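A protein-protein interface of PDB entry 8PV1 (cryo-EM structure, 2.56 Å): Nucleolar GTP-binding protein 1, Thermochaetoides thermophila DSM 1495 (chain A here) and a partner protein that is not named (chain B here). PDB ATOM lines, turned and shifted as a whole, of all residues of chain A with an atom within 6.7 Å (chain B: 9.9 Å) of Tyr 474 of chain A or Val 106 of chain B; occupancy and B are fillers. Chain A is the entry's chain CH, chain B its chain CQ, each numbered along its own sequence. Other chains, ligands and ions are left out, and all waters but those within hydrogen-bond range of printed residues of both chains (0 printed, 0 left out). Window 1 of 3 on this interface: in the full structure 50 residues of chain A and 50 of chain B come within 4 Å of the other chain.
The guanidinium group (NE) of Arg 103 of chain B is in hydrogen-bond range of the side-chain hydroxyl (OH) of Tyr 474 of chain A (2.9 Å).
The side-chain carboxylate (OE1) of Glu 465 of chain A lies within salt-bridge range of the guanidinium group (NH2) of Arg 103 of chain B (3.0 Å).
The side-chain carboxylate of Glu 464 of chain A is in salt-bridge range of the guanidinium group of Arg 103 of chain B (3.5 Å).
The side-chain hydroxyl of Ser 67 of chain B is in hydrogen-bond range of the side-chain carboxylate of Glu 464 of chain A (3.1 Å).
OE2 of Glu 465 of chain A is in salt-bridge range of NH1 of Arg 102 of chain B, at 3.7 Å.
The guanidinium group (NH1) of Arg 102 of chain B is in salt-bridge range of the side-chain carboxylate (OE2) of Glu 469 of chain A (3.0 Å).
The backbone carbonyl oxygen of Leu 468 of chain A sits at hydrogen-bond distance from the backbone NH of Phe 473 of chain A, at 2.9 Å.
The side-chain carboxylate of Asp 66 of chain B lies within salt-bridge range of the guanidinium group of Arg 103 of chain B (2.8 Å).
The side-chain carboxylate (OE1) of Glu 465 of chain A sits at hydrogen-bond distance from the side-chain hydroxyl (OH) of Tyr 474 of chain A (2.7 Å).
Among the printed residues, pairs that only touch across the chains: Glu 465 of chain A with Ile 99 of chain B (3.3 Å), Phe 473 of chain A with Val 106 of chain B (3.6 Å), Phe 473 of chain A with Lys 110 of chain B (3.7 Å), Tyr 474 of chain A with Arg 102 of chain B (3.2 Å), Tyr 474 of chain A with Val 106 of chain B (3.8 Å) and Glu 476 of chain A with Lys 109 of chain B (3.7 Å).
Glu 465 of chain A touches three residues of chain B.
No residue of chain B comes within 4 Å of Leu 468 of chain A.
Of chain B, only Arg 102 (3.2 Å), Arg 103 (2.9 Å) and Val 106 (3.8 Å) come within 4 Å of Tyr 474 of chain A.
No residue of chain B comes within 4 Å of Asp 475 of chain A.
Of the printed residues of chain B, Glu 476 of chain A touches Lys 109 (3.7 Å).
Of the printed residues of chain A, Ser 67 of chain B touches Glu 464.
Printed residues of chain A within 4 Å of Arg 103 of chain B: Glu 464, Glu 465 and Tyr 474.
Val 106 of chain B touches just these residues of chain A: Phe 473 (3.6 Å) and Tyr 474 (3.8 Å).
Printed residues of chain A within 4 Å of Lys 109 of chain B: Glu 476.
Of the printed residues of chain A, Lys 110 of chain B touches Phe 473 (3.7 Å).
The nearest residue of chain B that does not touch Tyr 474 of chain A is Ile 99 of chain B (4.7 Å).
The nearest residue of chain A that does not touch Val 106 of chain B is Asp 475 of chain A (6.2 Å).
Printed residues of chain A that touch a printed residue of chain B: Glu 464, Glu 465, Glu 469, Phe 473, Tyr 474 and Glu 476.
Of the 22 printed residues of chain B, 7 touch a printed residue of chain A.
Among the printed residues, 12 pairs touch across the chains.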
ATOM      1  N   GLU A 464       9.800  25.030  -8.708  1.00  0.00           N
ATOM      2  CA  GLU A 464       9.806  24.439  -7.373  1.00  0.00           C
ATOM      3  C   GLU A 464       9.291  23.003  -7.401  1.00  0.00           C
ATOM      4  O   GLU A 464       9.850  22.122  -6.738  1.00  0.00           O
ATOM      5  CB  GLU A 464       8.972  25.298  -6.425  1.00  0.00           C
ATOM      6  CG  GLU A 464       8.839  24.747  -5.019  1.00  0.00           C
ATOM      7  CD  GLU A 464       7.905  25.576  -4.160  1.00  0.00           C
ATOM      8  OE1 GLU A 464       7.278  26.512  -4.699  1.00  0.00           O
ATOM      9  OE2 GLU A 464       7.797  25.293  -2.949  1.00  0.00           O
ATOM     10  N   GLU A 465       8.238  22.752  -8.182  1.00  0.00           N
ATOM     11  CA  GLU A 465       7.670  21.411  -8.275  1.00  0.00           C
ATOM     12  C   GLU A 465       8.671  20.425  -8.861  1.00  0.00           C
ATOM     13  O   GLU A 465       8.859  19.327  -8.324  1.00  0.00           O
ATOM     14  CB  GLU A 465       6.391  21.444  -9.112  1.00  0.00           C
ATOM     15  CG  GLU A 465       5.642  20.118  -9.195  1.00  0.00           C
ATOM     16  CD  GLU A 465       4.842  19.788  -7.944  1.00  0.00           C
ATOM     17  OE1 GLU A 465       4.817  20.605  -7.000  1.00  0.00           O
ATOM     18  OE2 GLU A 465       4.228  18.702  -7.910  1.00  0.00           O
ATOM     19  N   GLU A 466       9.356  20.813  -9.941  1.00  0.00           N
ATOM     20  CA  GLU A 466      10.333  19.905 -10.536  1.00  0.00           C
ATOM     21  C   GLU A 466      11.562  19.758  -9.642  1.00  0.00           C
ATOM     22  O   GLU A 466      12.200  18.700  -9.621  1.00  0.00           O
ATOM     23  CB  GLU A 466      10.717  20.366 -11.946  1.00  0.00           C
ATOM     24  CG  GLU A 466      11.517  21.649 -12.030  1.00  0.00           C
ATOM     25  CD  GLU A 466      11.840  22.042 -13.456  1.00  0.00           C
ATOM     26  OE1 GLU A 466      11.396  21.335 -14.385  1.00  0.00           O
ATOM     27  OE2 GLU A 466      12.540  23.059 -13.650  1.00  0.00           O
ATOM     28  N   LEU A 468      11.519  19.732  -6.213  1.00  0.00           N
ATOM     29  CA  LEU A 468      11.169  18.733  -5.203  1.00  0.00           C
ATOM     30  C   LEU A 468      10.960  17.346  -5.807  1.00  0.00           C
ATOM     31  O   LEU A 468      11.218  16.335  -5.139  1.00  0.00           O
ATOM     32  CB  LEU A 468       9.945  19.173  -4.391  1.00  0.00           C
ATOM     33  CG  LEU A 468      10.105  20.209  -3.265  1.00  0.00           C
ATOM     34  CD1 LEU A 468      10.385  21.619  -3.693  1.00  0.00           C
ATOM     35  CD2 LEU A 468       8.850  20.201  -2.412  1.00  0.00           C
ATOM     36  N   GLU A 469      10.504  17.264  -7.062  1.00  0.00           N
ATOM     37  CA  GLU A 469      10.405  15.956  -7.709  1.00  0.00           C
ATOM     38  C   GLU A 469      11.780  15.340  -7.942  1.00  0.00           C
ATOM     39  O   GLU A 469      11.954  14.124  -7.791  1.00  0.00           O
ATOM     40  CB  GLU A 469       9.634  16.055  -9.024  1.00  0.00           C
ATOM     41  CG  GLU A 469       8.134  16.237  -8.861  1.00  0.00           C
ATOM     42  CD  GLU A 469       7.406  16.288 -10.189  1.00  0.00           C
ATOM     43  OE1 GLU A 469       8.085  16.313 -11.237  1.00  0.00           O
ATOM     44  OE2 GLU A 469       6.158  16.301 -10.187  1.00  0.00           O
ATOM     45  N   LYS A 470      12.766  16.154  -8.322  1.00  0.00           N
ATOM     46  CA  LYS A 470      14.129  15.643  -8.444  1.00  0.00           C
ATOM     47  C   LYS A 470      14.714  15.294  -7.081  1.00  0.00           C
ATOM     48  O   LYS A 470      15.435  14.300  -6.945  1.00  0.00           O
ATOM     49  CB  LYS A 470      15.017  16.656  -9.166  1.00  0.00           C
ATOM     50  CG  LYS A 470      14.674  16.851 -10.634  1.00  0.00           C
ATOM     51  CD  LYS A 470      15.206  18.178 -11.151  1.00  0.00           C
ATOM     52  CE  LYS A 470      14.610  18.521 -12.506  1.00  0.00           C
ATOM     53  NZ  LYS A 470      14.944  19.912 -12.921  1.00  0.00           N
ATOM     54  N   GLU A 471      14.417  16.097  -6.059  1.00  0.00           N
ATOM     55  CA  GLU A 471      14.934  15.840  -4.720  1.00  0.00           C
ATOM     56  C   GLU A 471      14.259  14.659  -4.035  1.00  0.00           C
ATOM     57  O   GLU A 471      14.789  14.169  -3.031  1.00  0.00           O
ATOM     58  CB  GLU A 471      14.786  17.088  -3.850  1.00  0.00           C
ATOM     59  CG  GLU A 471      15.851  18.144  -4.095  1.00  0.00           C
ATOM     60  CD  GLU A 471      15.524  19.467  -3.431  1.00  0.00           C
ATOM     61  OE1 GLU A 471      16.115  20.496  -3.825  1.00  0.00           O
ATOM     62  OE2 GLU A 471      14.677  19.480  -2.514  1.00  0.00           O
ATOM     63  N   GLY A 472      13.119  14.189  -4.537  1.00  0.00           N
ATOM     64  CA  GLY A 472      12.467  13.057  -3.911  1.00  0.00           C
ATOM     65  C   GLY A 472      11.528  13.419  -2.788  1.00  0.00           C
ATOM     66  O   GLY A 472      11.615  12.836  -1.705  1.00  0.00           O
ATOM     67  N   PHE A 473      10.641  14.388  -3.010  1.00  0.00           N
ATOM     68  CA  PHE A 473       9.725  14.816  -1.959  1.00  0.00           C
ATOM     69  C   PHE A 473       8.388  14.094  -2.087  1.00  0.00           C
ATOM     70  O   PHE A 473       7.685  13.890  -1.092  1.00  0.00           O
ATOM     71  CB  PHE A 473       9.616  16.352  -2.009  1.00  0.00           C
ATOM     72  CG  PHE A 473       8.496  16.968  -1.188  1.00  0.00           C
ATOM     73  CD1 PHE A 473       7.180  17.015  -1.643  1.00  0.00           C
ATOM     74  CD2 PHE A 473       8.784  17.530   0.047  1.00  0.00           C
ATOM     75  CE1 PHE A 473       6.188  17.596  -0.882  1.00  0.00           C
ATOM     76  CE2 PHE A 473       7.793  18.111   0.812  1.00  0.00           C
ATOM     77  CZ  PHE A 473       6.495  18.144   0.347  1.00  0.00           C
ATOM     78  N   TYR A 474       8.028  13.685  -3.302  1.00  0.00           N
ATOM     79  CA  TYR A 474       6.772  12.991  -3.546  1.00  0.00           C
ATOM     80  C   TYR A 474       6.941  11.483  -3.688  1.00  0.00           C
ATOM     81  O   TYR A 474       6.011  10.813  -4.148  1.00  0.00           O
ATOM     82  CB  TYR A 474       6.092  13.548  -4.798  1.00  0.00           C
ATOM     83  CG  TYR A 474       5.879  15.043  -4.778  1.00  0.00           C
ATOM     84  CD1 TYR A 474       4.785  15.596  -4.129  1.00  0.00           C
ATOM     85  CD2 TYR A 474       6.757  15.898  -5.429  1.00  0.00           C
ATOM     86  CE1 TYR A 474       4.578  16.961  -4.114  1.00  0.00           C
ATOM     87  CE2 TYR A 474       6.559  17.265  -5.419  1.00  0.00           C
ATOM     88  CZ  TYR A 474       5.469  17.790  -4.761  1.00  0.00           C
ATOM     89  OH  TYR A 474       5.267  19.149  -4.749  1.00  0.00           O
ATOM     90  N   ASP A 475       8.095  10.938  -3.314  1.00  0.00           N
ATOM     91  CA  ASP A 475       8.347   9.508  -3.460  1.00  0.00           C
ATOM     92  C   ASP A 475       7.569   8.723  -2.409  1.00  0.00           C
ATOM     93  O   ASP A 475       7.365   9.200  -1.288  1.00  0.00           O
ATOM     94  CB  ASP A 475       9.844   9.217  -3.363  1.00  0.00           C
ATOM     95  CG  ASP A 475      10.483   9.808  -2.119  1.00  0.00           C
ATOM     96  OD1 ASP A 475       9.820  10.593  -1.410  1.00  0.00           O
ATOM     97  OD2 ASP A 475      11.656   9.480  -1.845  1.00  0.00           O
ATOM     98  N   GLU A 476       7.126   7.522  -2.775  1.00  0.00           N
ATOM     99  CA  GLU A 476       6.363   6.661  -1.883  1.00  0.00           C
ATOM    100  C   GLU A 476       7.157   5.395  -1.590  1.00  0.00           C
ATOM    101  O   GLU A 476       7.823   4.854  -2.479  1.00  0.00           O
ATOM    102  CB  GLU A 476       5.007   6.306  -2.492  1.00  0.00           C
ATOM    103  CG  GLU A 476       4.139   7.511  -2.815  1.00  0.00           C
ATOM    104  CD  GLU A 476       2.753   7.122  -3.290  1.00  0.00           C
ATOM    105  OE1 GLU A 476       2.472   5.907  -3.376  1.00  0.00           O
ATOM    106  OE2 GLU A 476       1.946   8.030  -3.579  1.00  0.00           O
ATOM    107  N   MET B  63      -1.892  22.203   6.416  1.00  0.00           N
ATOM    108  CA  MET B  63      -0.726  22.707   5.707  1.00  0.00           C
ATOM    109  C   MET B  63      -0.885  24.206   5.489  1.00  0.00           C
ATOM    110  O   MET B  63      -1.725  24.638   4.693  1.00  0.00           O
ATOM    111  CB  MET B  63      -0.568  21.970   4.383  1.00  0.00           C
ATOM    112  CG  MET B  63       0.639  22.365   3.572  1.00  0.00           C
ATOM    113  SD  MET B  63       0.711  21.398   2.057  1.00  0.00           S
ATOM    114  CE  MET B  63      -0.645  22.122   1.147  1.00  0.00           C
ATOM    115  N   ASP B  66       3.177  26.908   2.587  1.00  0.00           N
ATOM    116  CA  ASP B  66       3.352  26.340   1.260  1.00  0.00           C
ATOM    117  C   ASP B  66       3.260  27.483   0.259  1.00  0.00           C
ATOM    118  O   ASP B  66       2.629  28.508   0.525  1.00  0.00           O
ATOM    119  CB  ASP B  66       2.297  25.259   0.966  1.00  0.00           C
ATOM    120  CG  ASP B  66       2.569  24.486  -0.320  1.00  0.00           C
ATOM    121  OD1 ASP B  66       3.556  24.782  -1.026  1.00  0.00           O
ATOM    122  OD2 ASP B  66       1.784  23.567  -0.628  1.00  0.00           O
ATOM    123  N   SER B  67       3.901  27.296  -0.896  1.00  0.00           N
ATOM    124  CA  SER B  67       3.878  28.331  -1.924  1.00  0.00           C
ATOM    125  C   SER B  67       2.533  28.377  -2.638  1.00  0.00           C
ATOM    126  O   SER B  67       2.164  29.405  -3.215  1.00  0.00           O
ATOM    127  CB  SER B  67       5.007  28.101  -2.925  1.00  0.00           C
ATOM    128  OG  SER B  67       6.273  28.228  -2.303  1.00  0.00           O
ATOM    129  N   THR B  68       1.785  27.273  -2.610  1.00  0.00           N
ATOM    130  CA  THR B  68       0.517  27.205  -3.325  1.00  0.00           C
ATOM    131  C   THR B  68      -0.603  27.970  -2.633  1.00  0.00           C
ATOM    132  O   THR B  68      -1.673  28.135  -3.228  1.00  0.00           O
ATOM    133  CB  THR B  68       0.099  25.746  -3.512  1.00  0.00           C
ATOM    134  OG1 THR B  68      -0.106  25.139  -2.231  1.00  0.00           O
ATOM    135  CG2 THR B  68       1.175  24.984  -4.254  1.00  0.00           C
ATOM    136  N   ARG B  95      -4.116  23.995 -12.158  1.00  0.00           N
ATOM    137  CA  ARG B  95      -2.829  23.371 -11.854  1.00  0.00           C
ATOM    138  C   ARG B  95      -2.442  23.566 -10.386  1.00  0.00           C
ATOM    139  O   ARG B  95      -1.892  22.654  -9.749  1.00  0.00           O
ATOM    140  CB  ARG B  95      -1.745  23.911 -12.786  1.00  0.00           C
ATOM    141  CG  ARG B  95      -0.378  23.314 -12.518  1.00  0.00           C
ATOM    142  CD  ARG B  95      -0.382  21.833 -12.869  1.00  0.00           C
ATOM    143  NE  ARG B  95       0.904  21.194 -12.622  1.00  0.00           N
ATOM    144  CZ  ARG B  95       1.886  21.115 -13.509  1.00  0.00           C
ATOM    145  NH1 ARG B  95       1.759  21.616 -14.727  1.00  0.00           N
ATOM    146  NH2 ARG B  95       3.024  20.519 -13.164  1.00  0.00           N
ATOM    147  N   ILE B  96      -2.745  24.741  -9.826  1.00  0.00           N
ATOM    148  CA  ILE B  96      -2.454  25.022  -8.422  1.00  0.00           C
ATOM    149  C   ILE B  96      -3.279  24.122  -7.512  1.00  0.00           C
ATOM    150  O   ILE B  96      -2.788  23.649  -6.481  1.00  0.00           O
ATOM    151  CB  ILE B  96      -2.683  26.519  -8.129  1.00  0.00           C
ATOM    152  CG1 ILE B  96      -1.534  27.350  -8.697  1.00  0.00           C
ATOM    153  CG2 ILE B  96      -2.833  26.802  -6.641  1.00  0.00           C
ATOM    154  CD1 ILE B  96      -1.887  28.797  -8.887  1.00  0.00           C
ATOM    155  N   GLU B  98      -4.263  21.050  -8.258  1.00  0.00           N
ATOM    156  CA  GLU B  98      -3.621  19.733  -8.306  1.00  0.00           C
ATOM    157  C   GLU B  98      -2.372  19.674  -7.421  1.00  0.00           C
ATOM    158  O   GLU B  98      -2.184  18.724  -6.640  1.00  0.00           O
ATOM    159  CB  GLU B  98      -3.266  19.373  -9.750  1.00  0.00           C
ATOM    160  CG  GLU B  98      -4.393  18.719 -10.526  1.00  0.00           C
ATOM    161  CD  GLU B  98      -4.363  19.068 -12.001  1.00  0.00           C
ATOM    162  OE1 GLU B  98      -3.257  19.289 -12.538  1.00  0.00           O
ATOM    163  OE2 GLU B  98      -5.443  19.118 -12.626  1.00  0.00           O
ATOM    164  N   ILE B  99      -1.518  20.697  -7.519  1.00  0.00           N
ATOM    165  CA  ILE B  99      -0.269  20.711  -6.756  1.00  0.00           C
ATOM    166  C   ILE B  99      -0.550  20.806  -5.258  1.00  0.00           C
ATOM    167  O   ILE B  99       0.101  20.136  -4.441  1.00  0.00           O
ATOM    168  CB  ILE B  99       0.632  21.858  -7.249  1.00  0.00           C
ATOM    169  CG1 ILE B  99       1.031  21.624  -8.706  1.00  0.00           C
ATOM    170  CG2 ILE B  99       1.870  21.990  -6.388  1.00  0.00           C
ATOM    171  CD1 ILE B  99       1.815  22.759  -9.313  1.00  0.00           C
ATOM    172  N   ARG B 100      -1.537  21.625  -4.880  1.00  0.00           N
ATOM    173  CA  ARG B 100      -1.935  21.755  -3.482  1.00  0.00           C
ATOM    174  C   ARG B 100      -2.440  20.435  -2.919  1.00  0.00           C
ATOM    175  O   ARG B 100      -2.103  20.075  -1.784  1.00  0.00           O
ATOM    176  CB  ARG B 100      -3.010  22.832  -3.349  1.00  0.00           C
ATOM    177  CG  ARG B 100      -3.439  23.112  -1.922  1.00  0.00           C
ATOM    178  CD  ARG B 100      -4.444  24.244  -1.862  1.00  0.00           C
ATOM    179  NE  ARG B 100      -4.891  24.495  -0.498  1.00  0.00           N
ATOM    180  CZ  ARG B 100      -5.757  25.438  -0.155  1.00  0.00           C
ATOM    181  NH1 ARG B 100      -6.294  26.245  -1.055  1.00  0.00           N
ATOM    182  NH2 ARG B 100      -6.087  25.579   1.126  1.00  0.00           N
ATOM    183  N   ALA B 101      -3.243  19.697  -3.698  1.00  0.00           N
ATOM    184  CA  ALA B 101      -3.730  18.398  -3.237  1.00  0.00           C
ATOM    185  C   ALA B 101      -2.584  17.418  -3.007  1.00  0.00           C
ATOM    186  O   ALA B 101      -2.552  16.708  -1.989  1.00  0.00           O
ATOM    187  CB  ALA B 101      -4.725  17.826  -4.244  1.00  0.00           C
ATOM    188  N   ARG B 102      -1.626  17.380  -3.937  1.00  0.00           N
ATOM    189  CA  ARG B 102      -0.517  16.433  -3.820  1.00  0.00           C
ATOM    190  C   ARG B 102       0.362  16.750  -2.608  1.00  0.00           C
ATOM    191  O   ARG B 102       0.731  15.852  -1.827  1.00  0.00           O
ATOM    192  CB  ARG B 102       0.283  16.453  -5.121  1.00  0.00           C
ATOM    193  CG  ARG B 102       1.413  15.465  -5.219  1.00  0.00           C
ATOM    194  CD  ARG B 102       2.037  15.559  -6.601  1.00  0.00           C
ATOM    195  NE  ARG B 102       3.168  14.658  -6.779  1.00  0.00           N
ATOM    196  CZ  ARG B 102       3.864  14.548  -7.902  1.00  0.00           C
ATOM    197  NH1 ARG B 102       3.563  15.264  -8.973  1.00  0.00           N
ATOM    198  NH2 ARG B 102       4.883  13.696  -7.954  1.00  0.00           N
ATOM    199  N   ARG B 103       0.665  18.034  -2.406  1.00  0.00           N
ATOM    200  CA  ARG B 103       1.481  18.423  -1.259  1.00  0.00           C
ATOM    201  C   ARG B 103       0.736  18.221   0.055  1.00  0.00           C
ATOM    202  O   ARG B 103       1.353  17.902   1.078  1.00  0.00           O
ATOM    203  CB  ARG B 103       1.941  19.870  -1.412  1.00  0.00           C
ATOM    204  CG  ARG B 103       2.840  20.080  -2.612  1.00  0.00           C
ATOM    205  CD  ARG B 103       3.400  21.481  -2.659  1.00  0.00           C
ATOM    206  NE  ARG B 103       4.305  21.655  -3.787  1.00  0.00           N
ATOM    207  CZ  ARG B 103       4.885  22.802  -4.110  1.00  0.00           C
ATOM    208  NH1 ARG B 103       4.668  23.907  -3.417  1.00  0.00           N
ATOM    209  NH2 ARG B 103       5.703  22.842  -5.158  1.00  0.00           N
ATOM    210  N   GLU B 104      -0.590  18.391   0.048  1.00  0.00           N
ATOM    211  CA  GLU B 104      -1.378  18.134   1.250  1.00  0.00           C
ATOM    212  C   GLU B 104      -1.342  16.660   1.630  1.00  0.00           C
ATOM    213  O   GLU B 104      -1.265  16.318   2.819  1.00  0.00           O
ATOM    214  CB  GLU B 104      -2.818  18.600   1.038  1.00  0.00           C
ATOM    215  CG  GLU B 104      -3.591  18.851   2.323  1.00  0.00           C
ATOM    216  CD  GLU B 104      -4.239  17.598   2.883  1.00  0.00           C
ATOM    217  OE1 GLU B 104      -4.681  16.746   2.086  1.00  0.00           O
ATOM    218  OE2 GLU B 104      -4.300  17.464   4.122  1.00  0.00           O
ATOM    219  N   ARG B 105      -1.413  15.770   0.634  1.00  0.00           N
ATOM    220  CA  ARG B 105      -1.314  14.341   0.921  1.00  0.00           C
ATOM    221  C   ARG B 105       0.049  13.986   1.510  1.00  0.00           C
ATOM    222  O   ARG B 105       0.142  13.194   2.466  1.00  0.00           O
ATOM    223  CB  ARG B 105      -1.588  13.531  -0.346  1.00  0.00           C
ATOM    224  CG  ARG B 105      -1.306  12.048  -0.201  1.00  0.00           C
ATOM    225  CD  ARG B 105      -1.929  11.249  -1.324  1.00  0.00           C
ATOM    226  NE  ARG B 105      -3.330  10.963  -1.049  1.00  0.00           N
ATOM    227  CZ  ARG B 105      -3.782   9.804  -0.591  1.00  0.00           C
ATOM    228  NH1 ARG B 105      -2.966   8.790  -0.352  1.00  0.00           N
ATOM    229  NH2 ARG B 105      -5.083   9.660  -0.363  1.00  0.00           N
ATOM    230  N   VAL B 106       1.118  14.582   0.968  1.00  0.00           N
ATOM    231  CA  VAL B 106       2.455  14.369   1.528  1.00  0.00           C
ATOM    232  C   VAL B 106       2.528  14.861   2.976  1.00  0.00           C
ATOM    233  O   VAL B 106       3.083  14.183   3.856  1.00  0.00           O
ATOM    234  CB  VAL B 106       3.513  15.049   0.638  1.00  0.00           C
ATOM    235  CG1 VAL B 106       4.868  15.042   1.305  1.00  0.00           C
ATOM    236  CG2 VAL B 106       3.593  14.350  -0.704  1.00  0.00           C
ATOM    237  N   PHE B 107       1.946  16.034   3.242  1.00  0.00           N
ATOM    238  CA  PHE B 107       1.920  16.594   4.593  1.00  0.00           C
ATOM    239  C   PHE B 107       1.198  15.667   5.568  1.00  0.00           C
ATOM    240  O   PHE B 107       1.657  15.460   6.700  1.00  0.00           O
ATOM    241  CB  PHE B 107       1.252  17.972   4.538  1.00  0.00           C
ATOM    242  CG  PHE B 107       1.130  18.661   5.865  1.00  0.00           C
ATOM    243  CD1 PHE B 107       2.172  19.422   6.362  1.00  0.00           C
ATOM    244  CD2 PHE B 107      -0.048  18.591   6.592  1.00  0.00           C
ATOM    245  CE1 PHE B 107       2.054  20.070   7.573  1.00  0.00           C
ATOM    246  CE2 PHE B 107      -0.168  19.234   7.804  1.00  0.00           C
ATOM    247  CZ  PHE B 107       0.882  19.976   8.294  1.00  0.00           C
ATOM    248  N   TYR B 108       0.082  15.078   5.134  1.00  0.00           N
ATOM    249  CA  TYR B 108      -0.669  14.177   6.004  1.00  0.00           C
ATOM    250  C   TYR B 108       0.116  12.900   6.295  1.00  0.00           C
ATOM    251  O   TYR B 108       0.066  12.366   7.412  1.00  0.00           O
ATOM    252  CB  TYR B 108      -2.026  13.855   5.378  1.00  0.00           C
ATOM    253  CG  TYR B 108      -2.935  13.063   6.288  1.00  0.00           C
ATOM    254  CD1 TYR B 108      -3.604  13.677   7.338  1.00  0.00           C
ATOM    255  CD2 TYR B 108      -3.131  11.705   6.096  1.00  0.00           C
ATOM    256  CE1 TYR B 108      -4.433  12.961   8.172  1.00  0.00           C
ATOM    257  CE2 TYR B 108      -3.964  10.982   6.925  1.00  0.00           C
ATOM    258  CZ  TYR B 108      -4.611  11.613   7.960  1.00  0.00           C
ATOM    259  OH  TYR B 108      -5.438  10.892   8.786  1.00  0.00           O
ATOM    260  N   LYS B 109       0.849  12.392   5.300  1.00  0.00           N
ATOM    261  CA  LYS B 109       1.678  11.210   5.542  1.00  0.00           C
ATOM    262  C   LYS B 109       2.804  11.490   6.536  1.00  0.00           C
ATOM    263  O   LYS B 109       3.103  10.647   7.398  1.00  0.00           O
ATOM    264  CB  LYS B 109       2.243  10.692   4.223  1.00  0.00           C
ATOM    265  CG  LYS B 109       1.194  10.091   3.309  1.00  0.00           C
ATOM    266  CD  LYS B 109       1.788   9.727   1.962  1.00  0.00           C
ATOM    267  CE  LYS B 109       2.723   8.535   2.073  1.00  0.00           C
ATOM    268  NZ  LYS B 109       3.218   8.102   0.737  1.00  0.00           N
ATOM    269  N   LYS B 110       3.447  12.658   6.432  1.00  0.00           N
ATOM    270  CA  LYS B 110       4.426  13.034   7.455  1.00  0.00           C
ATOM    271  C   LYS B 110       3.782  13.264   8.820  1.00  0.00           C
ATOM    272  O   LYS B 110       4.459  13.147   9.848  1.00  0.00           O
ATOM    273  CB  LYS B 110       5.253  14.247   7.014  1.00  0.00           C
ATOM    274  CG  LYS B 110       6.424  13.920   6.071  1.00  0.00           C
ATOM    275  CD  LYS B 110       6.078  13.543   4.647  1.00  0.00           C
ATOM    276  CE  LYS B 110       7.349  13.344   3.830  1.00  0.00           C
ATOM    277  NZ  LYS B 110       7.084  12.855   2.451  1.00  0.00           N
ATOM    278  N   ARG B 111       2.488  13.594   8.865  1.00  0.00           N
ATOM    279  CA  ARG B 111       1.807  13.585  10.161  1.00  0.00           C
ATOM    280  C   ARG B 111       1.620  12.166  10.696  1.00  0.00           C
ATOM    281  O   ARG B 111       1.716  11.944  11.908  1.00  0.00           O
ATOM    282  CB  ARG B 111       0.454  14.297  10.090  1.00  0.00           C
ATOM    283  CG  ARG B 111       0.531  15.761   9.703  1.00  0.00           C
ATOM    284  CD  ARG B 111      -0.497  16.596  10.449  1.00  0.00           C
ATOM    285  NE  ARG B 111      -1.870  16.194  10.174  1.00  0.00           N
ATOM    286  CZ  ARG B 111      -2.712  15.732  11.089  1.00  0.00           C
ATOM    287  NH1 ARG B 111      -2.348  15.590  12.352  1.00  0.00           N
ATOM    288  NH2 ARG B 111      -3.945  15.401  10.726  1.00  0.00           N
ATOM    289  N   MET B 112       1.353  11.195   9.819  1.00  0.00           N
ATOM    290  CA  MET B 112       1.018   9.840  10.250  1.00  0.00           C
ATOM    291  C   MET B 112       2.173   8.848  10.096  1.00  0.00           C
ATOM    292  O   MET B 112       1.929   7.647   9.943  1.00  0.00           O
ATOM    293  CB  MET B 112      -0.202   9.331   9.487  1.00  0.00           C
ATOM    294  CG  MET B 112      -1.378  10.279   9.507  1.00  0.00           C
ATOM    295  SD  MET B 112      -2.406  10.116  10.975  1.00  0.00           S
ATOM    296  CE  MET B 112      -2.586  11.837  11.428  1.00  0.00           C
ATOM    297  N   ALA B 113       3.416   9.340  10.083  1.00  0.00           N
ATOM    298  CA  ALA B 113       4.605   8.488   9.933  1.00  0.00           C
ATOM    299  C   ALA B 113       4.683   7.334  10.947  1.00  0.00           C
ATOM    300  O   ALA B 113       4.751   6.166  10.550  1.00  0.00           O
ATOM    301  CB  ALA B 113       5.862   9.350  10.029  1.00  0.00           C
